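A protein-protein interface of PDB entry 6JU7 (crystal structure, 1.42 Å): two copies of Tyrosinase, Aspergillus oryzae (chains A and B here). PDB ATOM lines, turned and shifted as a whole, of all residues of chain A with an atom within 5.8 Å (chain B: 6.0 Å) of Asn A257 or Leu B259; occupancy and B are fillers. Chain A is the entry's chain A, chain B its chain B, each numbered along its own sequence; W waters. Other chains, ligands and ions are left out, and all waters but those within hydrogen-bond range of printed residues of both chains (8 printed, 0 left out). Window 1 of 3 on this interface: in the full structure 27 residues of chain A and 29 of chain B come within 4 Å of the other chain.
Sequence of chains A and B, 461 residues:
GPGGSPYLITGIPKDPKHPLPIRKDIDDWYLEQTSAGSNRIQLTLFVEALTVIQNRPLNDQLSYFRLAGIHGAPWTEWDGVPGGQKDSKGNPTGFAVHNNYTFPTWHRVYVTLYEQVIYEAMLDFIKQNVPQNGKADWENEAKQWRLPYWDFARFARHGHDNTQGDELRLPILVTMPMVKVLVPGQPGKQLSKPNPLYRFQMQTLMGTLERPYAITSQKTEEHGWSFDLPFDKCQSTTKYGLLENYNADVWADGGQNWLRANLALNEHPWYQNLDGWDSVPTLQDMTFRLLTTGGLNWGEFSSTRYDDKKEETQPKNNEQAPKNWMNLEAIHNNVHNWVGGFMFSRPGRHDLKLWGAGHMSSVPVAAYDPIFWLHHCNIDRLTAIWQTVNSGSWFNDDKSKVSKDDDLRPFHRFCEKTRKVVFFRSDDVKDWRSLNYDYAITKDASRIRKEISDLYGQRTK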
ATOM      1  N   THR A 238      -3.403 -23.748 -16.591  1.00  0.00           N
ATOM      2  CA  THR A 238      -4.634 -24.520 -16.403  1.00  0.00           C
ATOM      3  C   THR A 238      -5.612 -24.229 -17.541  1.00  0.00           C
ATOM      4  O   THR A 238      -5.592 -23.118 -18.088  1.00  0.00           O
ATOM      5  CB  THR A 238      -5.243 -24.219 -15.029  1.00  0.00           C
ATOM      6  OG1 THR A 238      -6.430 -24.984 -14.796  1.00  0.00           O
ATOM      7  CG2 THR A 238      -5.644 -22.756 -14.862  1.00  0.00           C
ATOM      8  N   LYS A 239      -6.458 -25.187 -17.845  1.00  0.00           N
ATOM      9  CA  LYS A 239      -7.644 -25.045 -18.678  1.00  0.00           C
ATOM     10  C   LYS A 239      -8.850 -25.134 -17.733  1.00  0.00           C
ATOM     11  O   LYS A 239      -9.022 -26.198 -17.118  1.00  0.00           O
ATOM     12  CB  LYS A 239      -7.718 -26.089 -19.788  1.00  0.00           C
ATOM     13  CG  LYS A 239      -6.501 -26.114 -20.708  1.00  0.00           C
ATOM     14  CD  LYS A 239      -6.481 -27.402 -21.533  1.00  0.00           C
ATOM     15  CE  LYS A 239      -5.304 -27.490 -22.487  1.00  0.00           C
ATOM     16  NZ  LYS A 239      -4.007 -27.372 -21.758  1.00  0.00           N
ATOM     17  N   TYR A 240      -9.592 -24.049 -17.576  1.00  0.00           N
ATOM     18  CA  TYR A 240     -10.789 -23.916 -16.765  1.00  0.00           C
ATOM     19  C   TYR A 240     -10.586 -24.035 -15.266  1.00  0.00           C
ATOM     20  O   TYR A 240     -11.610 -23.964 -14.545  1.00  0.00           O
ATOM     21  CB  TYR A 240     -11.887 -24.924 -17.185  1.00  0.00           C
ATOM     22  CG  TYR A 240     -12.507 -24.611 -18.521  1.00  0.00           C
ATOM     23  CD1 TYR A 240     -11.886 -24.933 -19.724  1.00  0.00           C
ATOM     24  CD2 TYR A 240     -13.747 -23.977 -18.602  1.00  0.00           C
ATOM     25  CE1 TYR A 240     -12.468 -24.633 -20.947  1.00  0.00           C
ATOM     26  CE2 TYR A 240     -14.339 -23.662 -19.807  1.00  0.00           C
ATOM     27  CZ  TYR A 240     -13.692 -24.005 -20.990  1.00  0.00           C
ATOM     28  OH  TYR A 240     -14.311 -23.681 -22.176  1.00  0.00           O
ATOM     29  N   GLY A 241      -9.386 -24.191 -14.722  1.00  0.00           N
ATOM     30  CA  GLY A 241      -9.289 -24.503 -13.297  1.00  0.00           C
ATOM     31  C   GLY A 241      -9.336 -23.321 -12.358  1.00  0.00           C
ATOM     32  O   GLY A 241      -9.260 -23.562 -11.142  1.00  0.00           O
ATOM     33  N   LEU A 243     -11.489 -20.584 -10.551  1.00  0.00           N
ATOM     34  CA  LEU A 243     -12.887 -20.217 -10.293  1.00  0.00           C
ATOM     35  C   LEU A 243     -12.890 -19.219  -9.125  1.00  0.00           C
ATOM     36  O   LEU A 243     -12.123 -19.431  -8.171  1.00  0.00           O
ATOM     37  CB  LEU A 243     -13.733 -21.430  -9.914  1.00  0.00           C
ATOM     38  CG  LEU A 243     -14.250 -22.353 -11.022  1.00  0.00           C
ATOM     39  CD1 LEU A 243     -13.079 -22.963 -11.789  1.00  0.00           C
ATOM     40  CD2 LEU A 243     -15.157 -23.458 -10.463  1.00  0.00           C
ATOM     41  N   TYR A 246     -12.700 -19.924  -4.821  1.00  0.00           N
ATOM     42  CA  TYR A 246     -12.018 -21.166  -4.519  1.00  0.00           C
ATOM     43  C   TYR A 246     -10.708 -20.849  -3.808  1.00  0.00           C
ATOM     44  O   TYR A 246     -10.069 -19.825  -4.051  1.00  0.00           O
ATOM     45  CB  TYR A 246     -11.791 -21.991  -5.792  1.00  0.00           C
ATOM     46  CG  TYR A 246     -13.018 -22.785  -6.157  1.00  0.00           C
ATOM     47  CD1 TYR A 246     -14.242 -22.198  -6.453  1.00  0.00           C
ATOM     48  CD2 TYR A 246     -12.944 -24.176  -6.185  1.00  0.00           C
ATOM     49  CE1 TYR A 246     -15.343 -22.963  -6.775  1.00  0.00           C
ATOM     50  CE2 TYR A 246     -14.039 -24.967  -6.485  1.00  0.00           C
ATOM     51  CZ  TYR A 246     -15.242 -24.345  -6.784  1.00  0.00           C
ATOM     52  OH  TYR A 246     -16.336 -25.115  -7.106  1.00  0.00           O
ATOM     53  N   GLY A 254      -4.760 -25.771 -11.337  1.00  0.00           N
ATOM     54  CA  GLY A 254      -6.191 -25.972 -11.437  1.00  0.00           C
ATOM     55  C   GLY A 254      -6.585 -27.107 -12.354  1.00  0.00           C
ATOM     56  O   GLY A 254      -7.766 -27.409 -12.541  1.00  0.00           O
ATOM     57  N   GLY A 255      -5.588 -27.767 -12.960  1.00  0.00           N
ATOM     58  CA  GLY A 255      -5.830 -28.920 -13.793  1.00  0.00           C
ATOM     59  C   GLY A 255      -5.981 -28.601 -15.268  1.00  0.00           C
ATOM     60  O   GLY A 255      -6.125 -27.465 -15.717  1.00  0.00           O
ATOM     61  N   GLN A 256      -5.923 -29.680 -16.051  1.00  0.00           N
ATOM     62  CA  GLN A 256      -6.153 -29.629 -17.489  1.00  0.00           C
ATOM     63  C   GLN A 256      -7.559 -30.169 -17.723  1.00  0.00           C
ATOM     64  O   GLN A 256      -7.723 -31.364 -17.957  1.00  0.00           O
ATOM     65  CB  GLN A 256      -5.090 -30.455 -18.216  1.00  0.00           C
ATOM     66  CG  GLN A 256      -3.656 -30.054 -17.869  1.00  0.00           C
ATOM     67  CD  GLN A 256      -3.460 -28.537 -17.869  1.00  0.00           C
ATOM     68  OE1 GLN A 256      -3.829 -27.833 -18.805  1.00  0.00           O
ATOM     69  NE2 GLN A 256      -2.871 -28.043 -16.790  1.00  0.00           N
ATOM     70  N   ASN A 257      -8.549 -29.288 -17.625  1.00  0.00           N
ATOM     71  CA  ASN A 257      -9.942 -29.775 -17.620  1.00  0.00           C
ATOM     72  C   ASN A 257     -10.445 -29.883 -19.050  1.00  0.00           C
ATOM     73  O   ASN A 257     -11.280 -29.131 -19.540  1.00  0.00           O
ATOM     74  CB  ASN A 257     -10.787 -28.879 -16.716  1.00  0.00           C
ATOM     75  CG  ASN A 257     -10.232 -28.893 -15.294  1.00  0.00           C
ATOM     76  OD1 ASN A 257     -10.395 -29.906 -14.613  1.00  0.00           O
ATOM     77  ND2 ASN A 257      -9.564 -27.837 -14.873  1.00  0.00           N
ATOM     78  N   TRP A 258      -9.871 -30.878 -19.745  1.00  0.00           N
ATOM     79  CA  TRP A 258     -10.019 -30.992 -21.189  1.00  0.00           C
ATOM     80  C   TRP A 258     -11.436 -31.384 -21.584  1.00  0.00           C
ATOM     81  O   TRP A 258     -11.845 -31.119 -22.720  1.00  0.00           O
ATOM     82  CB  TRP A 258      -8.997 -31.976 -21.762  1.00  0.00           C
ATOM     83  CG  TRP A 258      -8.976 -33.369 -21.234  1.00  0.00           C
ATOM     84  CD1 TRP A 258      -8.229 -33.900 -20.208  1.00  0.00           C
ATOM     85  CD2 TRP A 258      -9.765 -34.458 -21.746  1.00  0.00           C
ATOM     86  NE1 TRP A 258      -8.514 -35.236 -20.056  1.00  0.00           N
ATOM     87  CE2 TRP A 258      -9.444 -35.605 -20.981  1.00  0.00           C
ATOM     88  CE3 TRP A 258     -10.692 -34.571 -22.777  1.00  0.00           C
ATOM     89  CZ2 TRP A 258     -10.040 -36.847 -21.220  1.00  0.00           C
ATOM     90  CZ3 TRP A 258     -11.283 -35.801 -23.011  1.00  0.00           C
ATOM     91  CH2 TRP A 258     -10.953 -36.930 -22.235  1.00  0.00           C
ATOM     92  N   LEU A 259     -12.207 -31.992 -20.679  1.00  0.00           N
ATOM     93  CA  LEU A 259     -13.586 -32.327 -21.035  1.00  0.00           C
ATOM     94  C   LEU A 259     -14.400 -31.059 -21.211  1.00  0.00           C
ATOM     95  O   LEU A 259     -15.318 -31.017 -22.050  1.00  0.00           O
ATOM     96  CB  LEU A 259     -14.262 -33.198 -19.967  1.00  0.00           C
ATOM     97  CG  LEU A 259     -13.684 -34.606 -19.809  1.00  0.00           C
ATOM     98  CD1 LEU A 259     -14.261 -35.238 -18.555  1.00  0.00           C
ATOM     99  CD2 LEU A 259     -13.980 -35.442 -21.049  1.00  0.00           C
ATOM    100  N   ARG A 260     -14.085 -30.048 -20.396  1.00  0.00           N
ATOM    101  CA  ARG A 260     -14.871 -28.815 -20.475  1.00  0.00           C
ATOM    102  C   ARG A 260     -14.479 -28.056 -21.731  1.00  0.00           C
ATOM    103  O   ARG A 260     -15.326 -27.462 -22.393  1.00  0.00           O
ATOM    104  CB  ARG A 260     -14.643 -27.974 -19.219  1.00  0.00           C
ATOM    105  CG  ARG A 260     -15.717 -26.919 -19.013  1.00  0.00           C
ATOM    106  CD  ARG A 260     -15.837 -26.536 -17.542  1.00  0.00           C
ATOM    107  NE  ARG A 260     -16.586 -27.592 -16.865  1.00  0.00           N
ATOM    108  CZ  ARG A 260     -17.347 -27.417 -15.797  1.00  0.00           C
ATOM    109  NH1 ARG A 260     -17.449 -26.228 -15.210  1.00  0.00           N
ATOM    110  NH2 ARG A 260     -17.991 -28.463 -15.307  1.00  0.00           N
ATOM    111  N   ALA A 261     -13.177 -28.082 -22.073  1.00  0.00           N
ATOM    112  CA  ALA A 261     -12.753 -27.462 -23.344  1.00  0.00           C
ATOM    113  C   ALA A 261     -13.450 -28.128 -24.525  1.00  0.00           C
ATOM    114  O   ALA A 261     -13.977 -27.463 -25.425  1.00  0.00           O
ATOM    115  CB  ALA A 261     -11.249 -27.588 -23.482  1.00  0.00           C
ATOM    116  N   ASN A 262     -13.502 -29.470 -24.536  1.00  0.00           N
ATOM    117  CA  ASN A 262     -14.193 -30.153 -25.626  1.00  0.00           C
ATOM    118  C   ASN A 262     -15.680 -29.788 -25.676  1.00  0.00           C
ATOM    119  O   ASN A 262     -16.279 -29.589 -26.742  1.00  0.00           O
ATOM    120  CB  ASN A 262     -14.025 -31.669 -25.489  1.00  0.00           C
ATOM    121  CG  ASN A 262     -12.640 -32.138 -25.893  1.00  0.00           C
ATOM    122  OD1 ASN A 262     -11.802 -31.323 -26.284  1.00  0.00           O
ATOM    123  ND2 ASN A 262     -12.404 -33.451 -25.795  1.00  0.00           N
ATOM    124  N   TRP A 355     -18.401 -23.136 -16.492  1.00  0.00           N
ATOM    125  CA  TRP A 355     -17.648 -22.270 -15.565  1.00  0.00           C
ATOM    126  C   TRP A 355     -16.183 -22.665 -15.474  1.00  0.00           C
ATOM    127  O   TRP A 355     -15.851 -23.864 -15.394  1.00  0.00           O
ATOM    128  CB  TRP A 355     -18.307 -22.387 -14.184  1.00  0.00           C
ATOM    129  CG  TRP A 355     -17.834 -21.508 -13.074  1.00  0.00           C
ATOM    130  CD1 TRP A 355     -17.128 -20.334 -13.145  1.00  0.00           C
ATOM    131  CD2 TRP A 355     -18.073 -21.735 -11.674  1.00  0.00           C
ATOM    132  NE1 TRP A 355     -16.913 -19.851 -11.874  1.00  0.00           N
ATOM    133  CE2 TRP A 355     -17.474 -20.688 -10.955  1.00  0.00           C
ATOM    134  CE3 TRP A 355     -18.725 -22.746 -10.962  1.00  0.00           C
ATOM    135  CZ2 TRP A 355     -17.506 -20.605  -9.565  1.00  0.00           C
ATOM    136  CZ3 TRP A 355     -18.758 -22.664  -9.579  1.00  0.00           C
ATOM    137  CH2 TRP A 355     -18.160 -21.604  -8.889  1.00  0.00           C
ATOM    138  N   GLY A 356     -15.324 -21.648 -15.451  1.00  0.00           N
ATOM    139  CA  GLY A 356     -13.940 -21.740 -15.071  1.00  0.00           C
ATOM    140  C   GLY A 356     -13.015 -21.028 -16.040  1.00  0.00           C
ATOM    141  O   GLY A 356     -13.266 -20.957 -17.246  1.00  0.00           O
ATOM    142  N   GLN B 256      -8.374 -36.015 -13.162  1.00  0.00           N
ATOM    143  CA  GLN B 256      -9.282 -35.791 -12.043  1.00  0.00           C
ATOM    144  C   GLN B 256     -10.193 -34.633 -12.436  1.00  0.00           C
ATOM    145  O   GLN B 256      -9.871 -33.477 -12.150  1.00  0.00           O
ATOM    146  CB  GLN B 256      -8.497 -35.476 -10.768  1.00  0.00           C
ATOM    147  CG  GLN B 256      -7.401 -36.488 -10.409  1.00  0.00           C
ATOM    148  CD  GLN B 256      -7.916 -37.914 -10.525  1.00  0.00           C
ATOM    149  OE1 GLN B 256      -8.974 -38.260  -9.979  1.00  0.00           O
ATOM    150  NE2 GLN B 256      -7.153 -38.727 -11.246  1.00  0.00           N
ATOM    151  N   ASN B 257     -11.278 -34.941 -13.139  1.00  0.00           N
ATOM    152  CA  ASN B 257     -12.096 -33.888 -13.763  1.00  0.00           C
ATOM    153  C   ASN B 257     -13.120 -33.395 -12.758  1.00  0.00           C
ATOM    154  O   ASN B 257     -14.327 -33.621 -12.852  1.00  0.00           O
ATOM    155  CB  ASN B 257     -12.687 -34.436 -15.061  1.00  0.00           C
ATOM    156  CG  ASN B 257     -11.546 -34.892 -15.971  1.00  0.00           C
ATOM    157  OD1 ASN B 257     -10.850 -34.015 -16.490  1.00  0.00           O
ATOM    158  ND2 ASN B 257     -11.358 -36.197 -16.149  1.00  0.00           N
ATOM    159  N   TRP B 258     -12.573 -32.715 -11.750  1.00  0.00           N
ATOM    160  CA  TRP B 258     -13.349 -32.342 -10.575  1.00  0.00           C
ATOM    161  C   TRP B 258     -14.434 -31.316 -10.869  1.00  0.00           C
ATOM    162  O   TRP B 258     -15.426 -31.212 -10.136  1.00  0.00           O
ATOM    163  CB  TRP B 258     -12.389 -31.867  -9.487  1.00  0.00           C
ATOM    164  CG  TRP B 258     -11.526 -30.678  -9.768  1.00  0.00           C
ATOM    165  CD1 TRP B 258     -10.239 -30.710 -10.225  1.00  0.00           C
ATOM    166  CD2 TRP B 258     -11.840 -29.295  -9.577  1.00  0.00           C
ATOM    167  NE1 TRP B 258      -9.754 -29.423 -10.354  1.00  0.00           N
ATOM    168  CE2 TRP B 258     -10.719 -28.538  -9.959  1.00  0.00           C
ATOM    169  CE3 TRP B 258     -12.983 -28.618  -9.132  1.00  0.00           C
ATOM    170  CZ2 TRP B 258     -10.675 -27.140  -9.910  1.00  0.00           C
ATOM    171  CZ3 TRP B 258     -12.938 -27.238  -9.089  1.00  0.00           C
ATOM    172  CH2 TRP B 258     -11.810 -26.496  -9.477  1.00  0.00           C
ATOM    173  N   LEU B 259     -14.293 -30.501 -11.920  1.00  0.00           N
ATOM    174  CA  LEU B 259     -15.372 -29.567 -12.231  1.00  0.00           C
ATOM    175  C   LEU B 259     -16.636 -30.315 -12.659  1.00  0.00           C
ATOM    176  O   LEU B 259     -17.755 -29.861 -12.380  1.00  0.00           O
ATOM    177  CB  LEU B 259     -14.971 -28.607 -13.348  1.00  0.00           C
ATOM    178  CG  LEU B 259     -13.842 -27.607 -13.082  1.00  0.00           C
ATOM    179  CD1 LEU B 259     -13.337 -27.051 -14.408  1.00  0.00           C
ATOM    180  CD2 LEU B 259     -14.351 -26.495 -12.192  1.00  0.00           C
ATOM    181  N   ARG B 260     -16.470 -31.439 -13.352  1.00  0.00           N
ATOM    182  CA  ARG B 260     -17.629 -32.203 -13.812  1.00  0.00           C
ATOM    183  C   ARG B 260     -18.270 -32.927 -12.648  1.00  0.00           C
ATOM    184  O   ARG B 260     -19.510 -33.027 -12.584  1.00  0.00           O
ATOM    185  CB  ARG B 260     -17.198 -33.142 -14.945  1.00  0.00           C
ATOM    186  CG  ARG B 260     -18.376 -33.729 -15.725  1.00  0.00           C
ATOM    187  CD  ARG B 260     -17.912 -34.155 -17.122  1.00  0.00           C
ATOM    188  NE  ARG B 260     -17.717 -32.940 -17.922  1.00  0.00           N
ATOM    189  CZ  ARG B 260     -17.747 -32.899 -19.249  1.00  0.00           C
ATOM    190  NH1 ARG B 260     -17.938 -34.013 -19.945  1.00  0.00           N
ATOM    191  NH2 ARG B 260     -17.584 -31.726 -19.843  1.00  0.00           N
ATOM    192  N   ALA B 261     -17.445 -33.400 -11.724  1.00  0.00           N
ATOM    193  CA  ALA B 261     -17.983 -34.020 -10.508  1.00  0.00           C
ATOM    194  C   ALA B 261     -18.798 -32.995  -9.725  1.00  0.00           C
ATOM    195  O   ALA B 261     -19.914 -33.291  -9.286  1.00  0.00           O
ATOM    196  CB  ALA B 261     -16.850 -34.550  -9.638  1.00  0.00           C
ATOM    197  N   ASN B 262     -18.244 -31.779  -9.578  1.00  0.00           N
ATOM    198  CA  ASN B 262     -19.007 -30.756  -8.845  1.00  0.00           C
ATOM    199  C   ASN B 262     -20.305 -30.439  -9.580  1.00  0.00           C
ATOM    200  O   ASN B 262     -21.356 -30.263  -8.948  1.00  0.00           O
ATOM    201  CB  ASN B 262     -18.167 -29.494  -8.675  1.00  0.00           C
ATOM    202  CG  ASN B 262     -17.080 -29.636  -7.625  1.00  0.00           C
ATOM    203  OD1 ASN B 262     -16.954 -30.673  -6.967  1.00  0.00           O
ATOM    204  ND2 ASN B 262     -16.278 -28.581  -7.489  1.00  0.00           N
ATOM    205  N   LEU B 263     -20.234 -30.352 -10.918  1.00  0.00           N
ATOM    206  CA  LEU B 263     -21.474 -30.075 -11.652  1.00  0.00           C
ATOM    207  C   LEU B 263     -22.508 -31.153 -11.367  1.00  0.00           C
ATOM    208  O   LEU B 263     -23.690 -30.854 -11.132  1.00  0.00           O
ATOM    209  CB  LEU B 263     -21.173 -29.978 -13.144  1.00  0.00           C
ATOM    210  CG  LEU B 263     -22.356 -29.671 -14.078  1.00  0.00           C
ATOM    211  CD1 LEU B 263     -22.898 -28.294 -13.776  1.00  0.00           C
ATOM    212  CD2 LEU B 263     -21.932 -29.811 -15.539  1.00  0.00           C
ATOM    213  N   ALA B 264     -22.088 -32.420 -11.359  1.00  0.00           N
ATOM    214  CA  ALA B 264     -23.043 -33.502 -11.097  1.00  0.00           C
ATOM    215  C   ALA B 264     -23.628 -33.430  -9.700  1.00  0.00           C
ATOM    216  O   ALA B 264     -24.831 -33.666  -9.511  1.00  0.00           O
ATOM    217  CB  ALA B 264     -22.366 -34.854 -11.306  1.00  0.00           C
HETATM  218  O   HOH W   1     -19.006 -29.731 -17.913  1.00  0.00           O
HETATM  219  O   HOH W   2     -12.070 -31.947 -17.790  1.00  0.00           O
HETATM  220  O   HOH W   3     -12.828 -31.029 -14.364  1.00  0.00           O
HETATM  221  O   HOH W   4      -6.746 -29.042  -9.843  1.00  0.00           O
HETATM  222  O   HOH W   5      -8.190 -33.774 -16.614  1.00  0.00           O
HETATM  223  O   HOH W   6      -8.484 -31.296 -13.293  1.00  0.00           O
HETATM  224  O   HOH W   7     -17.213 -26.307  -9.527  1.00  0.00           O
HETATM  225  O   HOH W   8     -16.639 -33.292 -22.775  1.00  0.00           O
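The side-chain amide nitrogen (ND2) of Asn B262 lies within hydrogen-bond range of the side-chain hydroxyl (OH) of Tyr A246 (3.5 Å). The backbone carbonyl oxygen of Leu A259 lies within hydrogen-bond range of the guanidinium group of Arg B260 (3.2 Å). O of Leu B259 lies within hydrogen-bond range of NH2 of Arg A260, 3.3 Å away.
The side-chain amide nitrogen (ND2) of Asn A257 is in hydrogen-bond range of the backbone carbonyl oxygen (O) of Lys A239, at 2.8 Å. The backbone carbonyl oxygen (O) of Gly A254 sits at hydrogen-bond distance from the side-chain amide nitrogen (ND2) of Asn A257 (3.0 Å). The backbone carbonyl oxygen (O) of Trp A355 is in hydrogen-bond range of the guanidinium group (NH1) of Arg A260 (2.9 Å).
CD1 of Leu B259 touches O of Tyr A240 (3.5 Å). Leu B259 touches Leu A243. CE2 of Tyr A246 touches CZ3 of Trp B258 (3.6 Å). O of Gly A254 touches NE1 of Trp B258, at 3.6 Å. Leu B259 touches Asn A257. Leu A259 touches Asn B257. Arg A260 touches Arg B260 (NH2 to N, 3.9 Å).
Of the printed residues of chain B, Asn A257 touches Leu B259 (3.7 Å). Leu B259 touches just these residues of chain A: Tyr A240, Leu A243, Asn A257 and Arg A260. Of the printed residues of chain B, Leu A259 touches Asn B257 and Arg B260. Of the printed residues of chain B, Tyr A240 touches Leu B259. Gln B256 touches none of the printed residues of chain A. Leu B263 touches none of the printed residues of chain A. The nearest residue of chain B that does not touch Asn A257 is Trp B258 (4.3 Å). The nearest residue of chain A that does not touch Leu B259 is Trp A355 (4.2 Å). The nearest printed residue of chain B that does not touch Gly A254 is Leu B259 (5.9 Å).
Of the 9 printed residues of chain B, 5 touch a printed residue of chain A. Printed residues of chain B that touch a printed residue of chain A: Asn B257, Trp B258, Leu B259, Arg B260 and Asn B262. Hydrophobic or aromatic side chains of chain B within 4 Å of the printed part of chain A: Trp B258 and Leu B259. Printed residues of chain A that touch a printed residue of chain B: Tyr A240, Leu A243, Tyr A246, Gly A254, Asn A257, Leu A259 and Arg A260. Hydrophobic or aromatic side chains of chain A that line the printed part of chain B: Tyr A240, Leu A243, Tyr A246 and Leu A259. Among the printed residues, 10 pairs touch across the chains. Among the printed residues, no Asp or Glu carboxylate lies within 4 Å of a Lys or Arg side-chain nitrogen of the other chain.
Asn A257 touches Leu B259, and with the chains exchanged Leu A259 touches Asn B257. Leu A259 touches Arg B260, and with the chains exchanged Arg A260 touches Leu B259. Arg B260 touches its own counterpart, Arg A260. 7 positions are printed for both chains. Of the 10 pairs that touch across the chains among the printed residues, 5 have their exchanged pair printed and touching as well.
Water W5 bridges OD1 of Asn B257 (2.7 Å) and O of Gln A256 (2.8 Å). Water W3 lies within hydrogen-bond range of OD1 of Asn A257 (2.7 Å), N of Leu B259 (2.9 Å), N of Trp B258 (3.1 Å) and O of Asn B257 (3.4 Å). Water W6 lies within hydrogen-bond range of OD1 of Asn A257 (2.7 Å) and O of Gln B256 (2.8 Å). Water W8 bridges O of Leu A259 and NH1 of Arg B260. Water W2 lies within hydrogen-bond range of OD1 of Asn B257 (2.7 Å), N of Leu A259 (2.9 Å), N of Trp A258 (3.1 Å) and O of Asn A257 (3.4 Å). Water W4 lies within hydrogen-bond range of the indole nitrogen of Trp B258 (3.1 Å) and the backbone carbonyl oxygen of Gly A254 (3.3 Å).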
